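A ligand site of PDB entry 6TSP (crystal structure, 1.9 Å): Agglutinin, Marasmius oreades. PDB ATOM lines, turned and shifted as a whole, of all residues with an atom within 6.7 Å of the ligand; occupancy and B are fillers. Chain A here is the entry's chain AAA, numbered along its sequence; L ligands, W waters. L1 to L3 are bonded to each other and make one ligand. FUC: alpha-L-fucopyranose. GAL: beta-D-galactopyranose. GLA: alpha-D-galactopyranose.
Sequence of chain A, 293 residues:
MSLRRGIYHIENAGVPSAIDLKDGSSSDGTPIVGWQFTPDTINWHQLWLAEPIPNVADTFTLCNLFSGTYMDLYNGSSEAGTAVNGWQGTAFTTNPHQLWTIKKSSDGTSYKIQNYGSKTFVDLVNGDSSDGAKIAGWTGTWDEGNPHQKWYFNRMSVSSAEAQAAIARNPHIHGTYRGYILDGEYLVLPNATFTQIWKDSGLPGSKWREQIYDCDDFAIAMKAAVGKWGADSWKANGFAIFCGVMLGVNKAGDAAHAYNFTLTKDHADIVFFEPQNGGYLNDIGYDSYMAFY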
ATOM      1  N   HIS A   9      12.998   2.228  15.397  1.00  0.00           N
ATOM      2  CA  HIS A   9      12.878   1.116  14.455  1.00  0.00           C
ATOM      3  C   HIS A   9      14.093   0.187  14.613  1.00  0.00           C
ATOM      4  O   HIS A   9      15.231   0.660  14.462  1.00  0.00           O
ATOM      5  CB  HIS A   9      12.747   1.667  13.008  1.00  0.00           C
ATOM      6  CG  HIS A   9      12.301   0.647  12.020  1.00  0.00           C
ATOM      7  ND1 HIS A   9      13.128   0.207  10.986  1.00  0.00           N
ATOM      8  CD2 HIS A   9      11.128  -0.020  11.882  1.00  0.00           C
ATOM      9  CE1 HIS A   9      12.503  -0.730  10.297  1.00  0.00           C
ATOM     10  NE2 HIS A   9      11.255  -0.835  10.784  1.00  0.00           N
ATOM     11  N   ASP A  20       9.111  -6.858  14.704  1.00  0.00           N
ATOM     12  CA  ASP A  20       7.747  -6.652  14.174  1.00  0.00           C
ATOM     13  C   ASP A  20       6.746  -7.386  15.079  1.00  0.00           C
ATOM     14  O   ASP A  20       6.938  -8.605  15.312  1.00  0.00           O
ATOM     15  CB  ASP A  20       7.637  -7.123  12.712  1.00  0.00           C
ATOM     16  CG  ASP A  20       6.306  -6.788  12.023  1.00  0.00           C
ATOM     17  OD1 ASP A  20       5.253  -7.365  12.444  1.00  0.00           O
ATOM     18  OD2 ASP A  20       6.352  -6.081  10.987  1.00  0.00           O
ATOM     19  N   LEU A  21       5.832  -6.649  15.693  1.00  0.00           N
ATOM     20  CA  LEU A  21       4.690  -7.252  16.407  1.00  0.00           C
ATOM     21  C   LEU A  21       3.661  -7.702  15.384  1.00  0.00           C
ATOM     22  O   LEU A  21       3.128  -6.822  14.652  1.00  0.00           O
ATOM     23  CB  LEU A  21       4.091  -6.215  17.375  1.00  0.00           C
ATOM     24  CG  LEU A  21       2.875  -6.695  18.172  1.00  0.00           C
ATOM     25  CD1 LEU A  21       3.220  -7.948  18.950  1.00  0.00           C
ATOM     26  CD2 LEU A  21       2.377  -5.602  19.107  1.00  0.00           C
ATOM     27  N   LYS A  22       3.471  -9.021  15.235  1.00  0.00           N
ATOM     28  CA  LYS A  22       2.836  -9.617  14.027  1.00  0.00           C
ATOM     29  C   LYS A  22       1.393  -9.098  13.892  1.00  0.00           C
ATOM     30  O   LYS A  22       0.642  -9.133  14.913  1.00  0.00           O
ATOM     31  CB  LYS A  22       2.849 -11.147  14.069  1.00  0.00           C
ATOM     32  CG  LYS A  22       2.749 -11.805  12.707  1.00  0.00           C
ATOM     33  CD  LYS A  22       2.848 -13.308  12.712  1.00  0.00           C
ATOM     34  CE  LYS A  22       2.736 -13.883  11.316  1.00  0.00           C
ATOM     35  NZ  LYS A  22       2.918 -15.354  11.307  1.00  0.00           N
ATOM     36  N   ASP A  23       1.088  -8.487  12.746  1.00  0.00           N
ATOM     37  CA  ASP A  23      -0.227  -7.867  12.436  1.00  0.00           C
ATOM     38  C   ASP A  23      -0.557  -6.760  13.443  1.00  0.00           C
ATOM     39  O   ASP A  23      -1.699  -6.234  13.392  1.00  0.00           O
ATOM     40  CB  ASP A  23      -1.345  -8.896  12.396  1.00  0.00           C
ATOM     41  CG  ASP A  23      -2.519  -8.487  11.526  1.00  0.00           C
ATOM     42  OD1 ASP A  23      -2.268  -7.893  10.448  1.00  0.00           O
ATOM     43  OD2 ASP A  23      -3.671  -8.710  11.936  1.00  0.00           O
ATOM     44  N   GLY A  24       0.429  -6.329  14.217  1.00  0.00           N
ATOM     45  CA  GLY A  24       0.267  -5.223  15.168  1.00  0.00           C
ATOM     46  C   GLY A  24      -0.850  -5.512  16.176  1.00  0.00           C
ATOM     47  O   GLY A  24      -1.334  -4.557  16.801  1.00  0.00           O
ATOM     48  N   VAL A  33       8.414 -10.932  15.640  1.00  0.00           N
ATOM     49  CA  VAL A  33       9.077 -11.664  14.538  1.00  0.00           C
ATOM     50  C   VAL A  33       9.999 -10.700  13.804  1.00  0.00           C
ATOM     51  O   VAL A  33       9.737  -9.469  13.850  1.00  0.00           O
ATOM     52  CB  VAL A  33       8.046 -12.305  13.565  1.00  0.00           C
ATOM     53  CG1 VAL A  33       7.267 -13.413  14.232  1.00  0.00           C
ATOM     54  CG2 VAL A  33       7.102 -11.255  12.959  1.00  0.00           C
ATOM     55  N   TRP A  35      10.798  -9.025  10.157  1.00  0.00           N
ATOM     56  CA  TRP A  35       9.994  -8.643   8.982  1.00  0.00           C
ATOM     57  C   TRP A  35      10.706  -7.523   8.208  1.00  0.00           C
ATOM     58  O   TRP A  35      11.237  -6.604   8.859  1.00  0.00           O
ATOM     59  CB  TRP A  35       8.581  -8.219   9.420  1.00  0.00           C
ATOM     60  CG  TRP A  35       7.550  -8.461   8.375  1.00  0.00           C
ATOM     61  CD1 TRP A  35       7.366  -7.749   7.219  1.00  0.00           C
ATOM     62  CD2 TRP A  35       6.609  -9.539   8.338  1.00  0.00           C
ATOM     63  NE1 TRP A  35       6.323  -8.270   6.506  1.00  0.00           N
ATOM     64  CE2 TRP A  35       5.841  -9.381   7.152  1.00  0.00           C
ATOM     65  CE3 TRP A  35       6.315 -10.602   9.196  1.00  0.00           C
ATOM     66  CZ2 TRP A  35       4.812 -10.250   6.811  1.00  0.00           C
ATOM     67  CZ3 TRP A  35       5.302 -11.481   8.844  1.00  0.00           C
ATOM     68  CH2 TRP A  35       4.554 -11.291   7.674  1.00  0.00           C
ATOM     69  N   GLN A  36      10.672  -7.604   6.884  1.00  0.00           N
ATOM     70  CA  GLN A  36      11.303  -6.609   6.019  1.00  0.00           C
ATOM     71  C   GLN A  36      10.541  -5.294   6.147  1.00  0.00           C
ATOM     72  O   GLN A  36       9.448  -5.299   6.795  1.00  0.00           O
ATOM     73  CB  GLN A  36      11.345  -7.106   4.543  1.00  0.00           C
ATOM     74  CG  GLN A  36       9.997  -7.111   3.837  1.00  0.00           C
ATOM     75  CD  GLN A  36      10.102  -7.609   2.406  1.00  0.00           C
ATOM     76  OE1 GLN A  36      10.669  -6.934   1.545  1.00  0.00           O
ATOM     77  NE2 GLN A  36       9.685  -8.856   2.177  1.00  0.00           N
ATOM     78  N   PHE A  37      11.173  -4.223   5.812  1.00  0.00           N
ATOM     79  CA  PHE A  37      10.672  -2.858   6.101  1.00  0.00           C
ATOM     80  C   PHE A  37      10.916  -1.974   4.880  1.00  0.00           C
ATOM     81  O   PHE A  37      11.714  -2.359   3.986  1.00  0.00           O
ATOM     82  CB  PHE A  37      11.349  -2.299   7.345  1.00  0.00           C
ATOM     83  CG  PHE A  37      12.850  -2.373   7.339  1.00  0.00           C
ATOM     84  CD1 PHE A  37      13.502  -3.435   7.928  1.00  0.00           C
ATOM     85  CD2 PHE A  37      13.606  -1.267   6.966  1.00  0.00           C
ATOM     86  CE1 PHE A  37      14.897  -3.460   8.000  1.00  0.00           C
ATOM     87  CE2 PHE A  37      14.988  -1.284   7.072  1.00  0.00           C
ATOM     88  CZ  PHE A  37      15.622  -2.398   7.546  1.00  0.00           C
ATOM     89  N   THR A  38      10.216  -0.858   4.814  1.00  0.00           N
ATOM     90  CA  THR A  38      10.441   0.172   3.774  1.00  0.00           C
ATOM     91  C   THR A  38      10.953   1.452   4.444  1.00  0.00           C
ATOM     92  O   THR A  38      10.278   2.020   5.297  1.00  0.00           O
ATOM     93  CB  THR A  38       9.148   0.410   2.973  1.00  0.00           C
ATOM     94  OG1 THR A  38       8.623  -0.853   2.573  1.00  0.00           O
ATOM     95  CG2 THR A  38       9.360   1.287   1.765  1.00  0.00           C
ATOM     96  N   PRO A  39      12.153   1.938   4.068  1.00  0.00           N
ATOM     97  CA  PRO A  39      12.691   3.180   4.627  1.00  0.00           C
ATOM     98  C   PRO A  39      11.850   4.407   4.250  1.00  0.00           C
ATOM     99  O   PRO A  39      11.252   4.404   3.204  1.00  0.00           O
ATOM    100  CB  PRO A  39      14.097   3.310   3.984  1.00  0.00           C
ATOM    101  CG  PRO A  39      14.382   1.913   3.407  1.00  0.00           C
ATOM    102  CD  PRO A  39      13.025   1.343   3.076  1.00  0.00           C
ATOM    103  N   THR A  41       9.174   5.377   5.362  1.00  0.00           N
ATOM    104  CA  THR A  41       7.721   5.223   5.621  1.00  0.00           C
ATOM    105  C   THR A  41       7.484   5.199   7.112  1.00  0.00           C
ATOM    106  O   THR A  41       8.461   4.960   7.874  1.00  0.00           O
ATOM    107  CB  THR A  41       7.141   3.958   4.966  1.00  0.00           C
ATOM    108  OG1 THR A  41       7.677   2.822   5.666  1.00  0.00           O
ATOM    109  CG2 THR A  41       7.462   3.843   3.499  1.00  0.00           C
ATOM    110  N   ILE A  42       6.230   5.186   7.493  1.00  0.00           N
ATOM    111  CA  ILE A  42       5.787   4.637   8.774  1.00  0.00           C
ATOM    112  C   ILE A  42       5.723   3.110   8.638  1.00  0.00           C
ATOM    113  O   ILE A  42       4.894   2.625   7.860  1.00  0.00           O
ATOM    114  CB  ILE A  42       4.421   5.241   9.155  1.00  0.00           C
ATOM    115  CG1 ILE A  42       4.498   6.758   9.334  1.00  0.00           C
ATOM    116  CG2 ILE A  42       3.866   4.555  10.389  1.00  0.00           C
ATOM    117  CD1 ILE A  42       5.487   7.212  10.417  1.00  0.00           C
ATOM    118  N   ASN A  43       6.572   2.402   9.372  1.00  0.00           N
ATOM    119  CA  ASN A  43       6.477   0.902   9.496  1.00  0.00           C
ATOM    120  C   ASN A  43       5.585   0.576  10.685  1.00  0.00           C
ATOM    121  O   ASN A  43       6.087   0.579  11.867  1.00  0.00           O
ATOM    122  CB  ASN A  43       7.844   0.251   9.592  1.00  0.00           C
ATOM    123  CG  ASN A  43       8.664   0.457   8.337  1.00  0.00           C
ATOM    124  OD1 ASN A  43       8.437  -0.207   7.323  1.00  0.00           O
ATOM    125  ND2 ASN A  43       9.578   1.432   8.379  1.00  0.00           N
ATOM    126  N   TRP A  44       4.315   0.320  10.418  1.00  0.00           N
ATOM    127  CA  TRP A  44       3.217   0.505  11.378  1.00  0.00           C
ATOM    128  C   TRP A  44       3.390  -0.450  12.583  1.00  0.00           C
ATOM    129  O   TRP A  44       2.911  -0.101  13.700  1.00  0.00           O
ATOM    130  CB  TRP A  44       1.887   0.295  10.687  1.00  0.00           C
ATOM    131  CG  TRP A  44       1.373   1.531  10.045  1.00  0.00           C
ATOM    132  CD1 TRP A  44       1.469   1.880   8.732  1.00  0.00           C
ATOM    133  CD2 TRP A  44       0.775   2.650  10.707  1.00  0.00           C
ATOM    134  NE1 TRP A  44       0.942   3.120   8.532  1.00  0.00           N
ATOM    135  CE2 TRP A  44       0.506   3.617   9.721  1.00  0.00           C
ATOM    136  CE3 TRP A  44       0.406   2.909  12.028  1.00  0.00           C
ATOM    137  CZ2 TRP A  44      -0.112   4.827  10.020  1.00  0.00           C
ATOM    138  CZ3 TRP A  44      -0.169   4.118  12.335  1.00  0.00           C
ATOM    139  CH2 TRP A  44      -0.437   5.058  11.338  1.00  0.00           C
ATOM    140  N   HIS A  45       3.931  -1.652  12.349  1.00  0.00           N
ATOM    141  CA  HIS A  45       3.987  -2.723  13.382  1.00  0.00           C
ATOM    142  C   HIS A  45       5.384  -2.794  13.998  1.00  0.00           C
ATOM    143  O   HIS A  45       5.611  -3.715  14.908  1.00  0.00           O
ATOM    144  CB  HIS A  45       3.553  -4.065  12.777  1.00  0.00           C
ATOM    145  CG  HIS A  45       2.180  -4.042  12.222  1.00  0.00           C
ATOM    146  ND1 HIS A  45       1.747  -4.951  11.262  1.00  0.00           N
ATOM    147  CD2 HIS A  45       1.148  -3.192  12.430  1.00  0.00           C
ATOM    148  CE1 HIS A  45       0.496  -4.654  10.925  1.00  0.00           C
ATOM    149  NE2 HIS A  45       0.133  -3.551  11.593  1.00  0.00           N
ATOM    150  N   GLN A  46       6.249  -1.847  13.666  1.00  0.00           N
ATOM    151  CA  GLN A  46       7.736  -1.989  13.839  1.00  0.00           C
ATOM    152  C   GLN A  46       8.326  -0.786  14.624  1.00  0.00           C
ATOM    153  O   GLN A  46       9.543  -0.566  14.534  1.00  0.00           O
ATOM    154  CB  GLN A  46       8.409  -2.124  12.486  1.00  0.00           C
ATOM    155  CG  GLN A  46       8.098  -3.416  11.772  1.00  0.00           C
ATOM    156  CD  GLN A  46       8.723  -3.477  10.386  1.00  0.00           C
ATOM    157  OE1 GLN A  46       9.468  -2.582   9.986  1.00  0.00           O
ATOM    158  NE2 GLN A  46       8.431  -4.551   9.648  1.00  0.00           N
ATOM    159  N   PHE A  66       2.086   1.046  18.066  1.00  0.00           N
ATOM    160  CA  PHE A  66       0.772   0.795  17.438  1.00  0.00           C
ATOM    161  C   PHE A  66      -0.143   0.048  18.421  1.00  0.00           C
ATOM    162  O   PHE A  66      -1.324   0.445  18.561  1.00  0.00           O
ATOM    163  CB  PHE A  66       0.935   0.002  16.146  1.00  0.00           C
ATOM    164  CG  PHE A  66      -0.365  -0.274  15.432  1.00  0.00           C
ATOM    165  CD1 PHE A  66      -1.080   0.766  14.833  1.00  0.00           C
ATOM    166  CD2 PHE A  66      -0.932  -1.556  15.436  1.00  0.00           C
ATOM    167  CE1 PHE A  66      -2.302   0.509  14.209  1.00  0.00           C
ATOM    168  CE2 PHE A  66      -2.154  -1.800  14.818  1.00  0.00           C
ATOM    169  CZ  PHE A  66      -2.838  -0.765  14.200  1.00  0.00           C
ATOM    170  N   ASP A 131      10.142 -13.190   6.265  1.00  0.00           N
ATOM    171  CA  ASP A 131       9.054 -12.441   6.928  1.00  0.00           C
ATOM    172  C   ASP A 131       8.303 -13.391   7.878  1.00  0.00           C
ATOM    173  O   ASP A 131       7.842 -14.411   7.417  1.00  0.00           O
ATOM    174  CB  ASP A 131       8.134 -11.801   5.896  1.00  0.00           C
ATOM    175  CG  ASP A 131       8.771 -10.621   5.155  1.00  0.00           C
ATOM    176  OD1 ASP A 131       9.749 -10.097   5.670  1.00  0.00           O
ATOM    177  OD2 ASP A 131       8.313 -10.313   4.038  1.00  0.00           O
HETATM  178  C1  FUC L   1       2.013  -3.129   5.873  1.00  0.00           C
HETATM  179  C2  FUC L   1       1.429  -2.872   4.521  1.00  0.00           C
HETATM  180  C3  FUC L   1      -0.089  -2.969   4.549  1.00  0.00           C
HETATM  181  C4  FUC L   1      -0.677  -2.139   5.697  1.00  0.00           C
HETATM  182  C5  FUC L   1       0.003  -2.506   7.009  1.00  0.00           C
HETATM  183  C6  FUC L   1      -0.517  -1.688   8.210  1.00  0.00           C
HETATM  184  O2  FUC L   1       1.944  -3.845   3.596  1.00  0.00           O
HETATM  185  O3  FUC L   1      -0.571  -2.499   3.320  1.00  0.00           O
HETATM  186  O4  FUC L   1      -0.518  -0.759   5.425  1.00  0.00           O
HETATM  187  O5  FUC L   1       1.409  -2.295   6.865  1.00  0.00           O
HETATM  188  C1  GAL L   2       1.428  -6.150   7.779  1.00  0.00           C
HETATM  189  C2  GAL L   2       2.316  -4.977   7.405  1.00  0.00           C
HETATM  190  C3  GAL L   2       3.799  -5.406   7.255  1.00  0.00           C
HETATM  191  C4  GAL L   2       4.227  -6.152   8.532  1.00  0.00           C
HETATM  192  C5  GAL L   2       3.220  -7.315   8.766  1.00  0.00           C
HETATM  193  C6  GAL L   2       3.578  -8.204   9.958  1.00  0.00           C
HETATM  194  O1  GAL L   2       0.127  -5.635   8.013  1.00  0.00           O
HETATM  195  O2  GAL L   2       1.840  -4.432   6.198  1.00  0.00           O
HETATM  196  O3  GAL L   2       4.555  -4.284   7.009  1.00  0.00           O
HETATM  197  O4  GAL L   2       4.323  -5.273   9.679  1.00  0.00           O
HETATM  198  O5  GAL L   2       1.907  -6.774   8.953  1.00  0.00           O
HETATM  199  O6  GAL L   2       3.064  -7.639  11.194  1.00  0.00           O
HETATM  200  C1  GLA L   3       5.913  -4.409   6.821  1.00  0.00           C
HETATM  201  C2  GLA L   3       6.603  -3.070   6.546  1.00  0.00           C
HETATM  202  C3  GLA L   3       6.313  -2.554   5.097  1.00  0.00           C
HETATM  203  C4  GLA L   3       6.554  -3.669   4.102  1.00  0.00           C
HETATM  204  C5  GLA L   3       5.722  -4.880   4.516  1.00  0.00           C
HETATM  205  C6  GLA L   3       5.796  -6.018   3.489  1.00  0.00           C
HETATM  206  O2  GLA L   3       6.165  -2.129   7.517  1.00  0.00           O
HETATM  207  O3  GLA L   3       7.135  -1.438   4.796  1.00  0.00           O
HETATM  208  O4  GLA L   3       7.962  -4.004   4.033  1.00  0.00           O
HETATM  209  O5  GLA L   3       6.202  -5.341   5.760  1.00  0.00           O
HETATM  210  O6  GLA L   3       5.091  -7.162   4.012  1.00  0.00           O
HETATM  211  O   HOH W   1       4.932  -2.543   9.796  1.00  0.00           O
HETATM  212  O   HOH W   2       2.286  -6.496   3.885  1.00  0.00           O
HETATM  213  O   HOH W   3      -2.427   1.238   5.844  1.00  0.00           O
HETATM  214  O   HOH W   4       0.004  -8.907   9.206  1.00  0.00           O
HETATM  215  O   HOH W   5       5.909   0.708   5.611  1.00  0.00           O
HETATM  216  O   HOH W   6       3.924  -0.372   7.492  1.00  0.00           O
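O of Leu 21 touches O6 of GAL L2, 3.6 Å away. CA of Lys 22 touches O6 of GAL L2, at 3.5 Å. CA of Phe 37 touches O4 of GLA L3, at 3.6 Å. CB of Trp 44 touches C6 of FUC L1, at 3.98 Å. NE2 of Gln 46 touches C1 of GLA L3, at 3.8 Å. Hydrophobic or aromatic side chains within 4 Å of the ligand: Trp 35, Trp 44 and His 45. The nearest printed residue that does not touch the ligand is Gly 24 (4.2 Å).
O6 of GAL L2 lies within hydrogen-bond range of N of Asp 23 (2.7 Å). N of Thr 38 is in hydrogen-bond range of O3 of GLA L3 (3.1 Å). An oxygen (O3) of GLA L3 is in hydrogen-bond range of the side-chain hydroxyl (OG1) of Thr 38. OD1 of Asp 20 is in hydrogen-bond range of O6 of GAL L2 (2.5 Å). A ring nitrogen (ND1) of His 45 is in hydrogen-bond range of an oxygen (O5) of GAL L2. OD1 of Asn 43 is in hydrogen-bond range of O2 of GLA L3 (3.0 Å). The backbone carbonyl oxygen (O) of Gln 36 is in hydrogen-bond range of an oxygen (O4) of GLA L3. O6 of GLA L3 lies within hydrogen-bond range of NE1 of Trp 35.
NE2 of Gln 36 is in hydrogen-bond range of OD2 of Asp 131. The side-chain amide oxygen (OD1) of Asn 43 lies within hydrogen-bond range of the backbone NH (N) of Thr 38. OD2 of Asp 20 lies within hydrogen-bond range of NE2 of Gln 46, 2.9 Å away. The backbone carbonyl oxygen (O) of Thr 38 is in hydrogen-bond range of the side-chain hydroxyl (OG1) of Thr 41 (2.7 Å). A ring nitrogen (NE2) of His 9 lies within hydrogen-bond range of the side-chain amide oxygen of Gln 46. The backbone carbonyl oxygen (O) of Gln 36 lies within hydrogen-bond range of the side-chain amide nitrogen (NE2) of Gln 46, 3.1 Å away. The backbone NH (N) of Val 33 lies within hydrogen-bond range of the backbone carbonyl oxygen (O) of Asp 20 (2.8 Å). The backbone NH (N) of Leu 21 lies within hydrogen-bond range of the backbone carbonyl oxygen (O) of His 45, 3.0 Å away.
Water W5 lies within hydrogen-bond range of O3 of GLA L3 (2.6 Å), OG1 of Thr 41 (2.8 Å), O of Ile 42 (3.1 Å) and OD1 of Asn 43 (3.2 Å). Water W1 lies within hydrogen-bond range of O2 of GLA L3, N of His 45 and N of Trp 44. Water W6 lies within hydrogen-bond range of an oxygen (O2) of GLA L3 (2.8 Å), the backbone NH of Trp 44 (3.0 Å) and the backbone carbonyl oxygen of Ile 42 (3.2 Å). Water W4 bridges the side-chain carboxylate (OD1) of Asp 23 (2.8 Å) and an oxygen (O5) of GAL L2 (2.9 Å).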
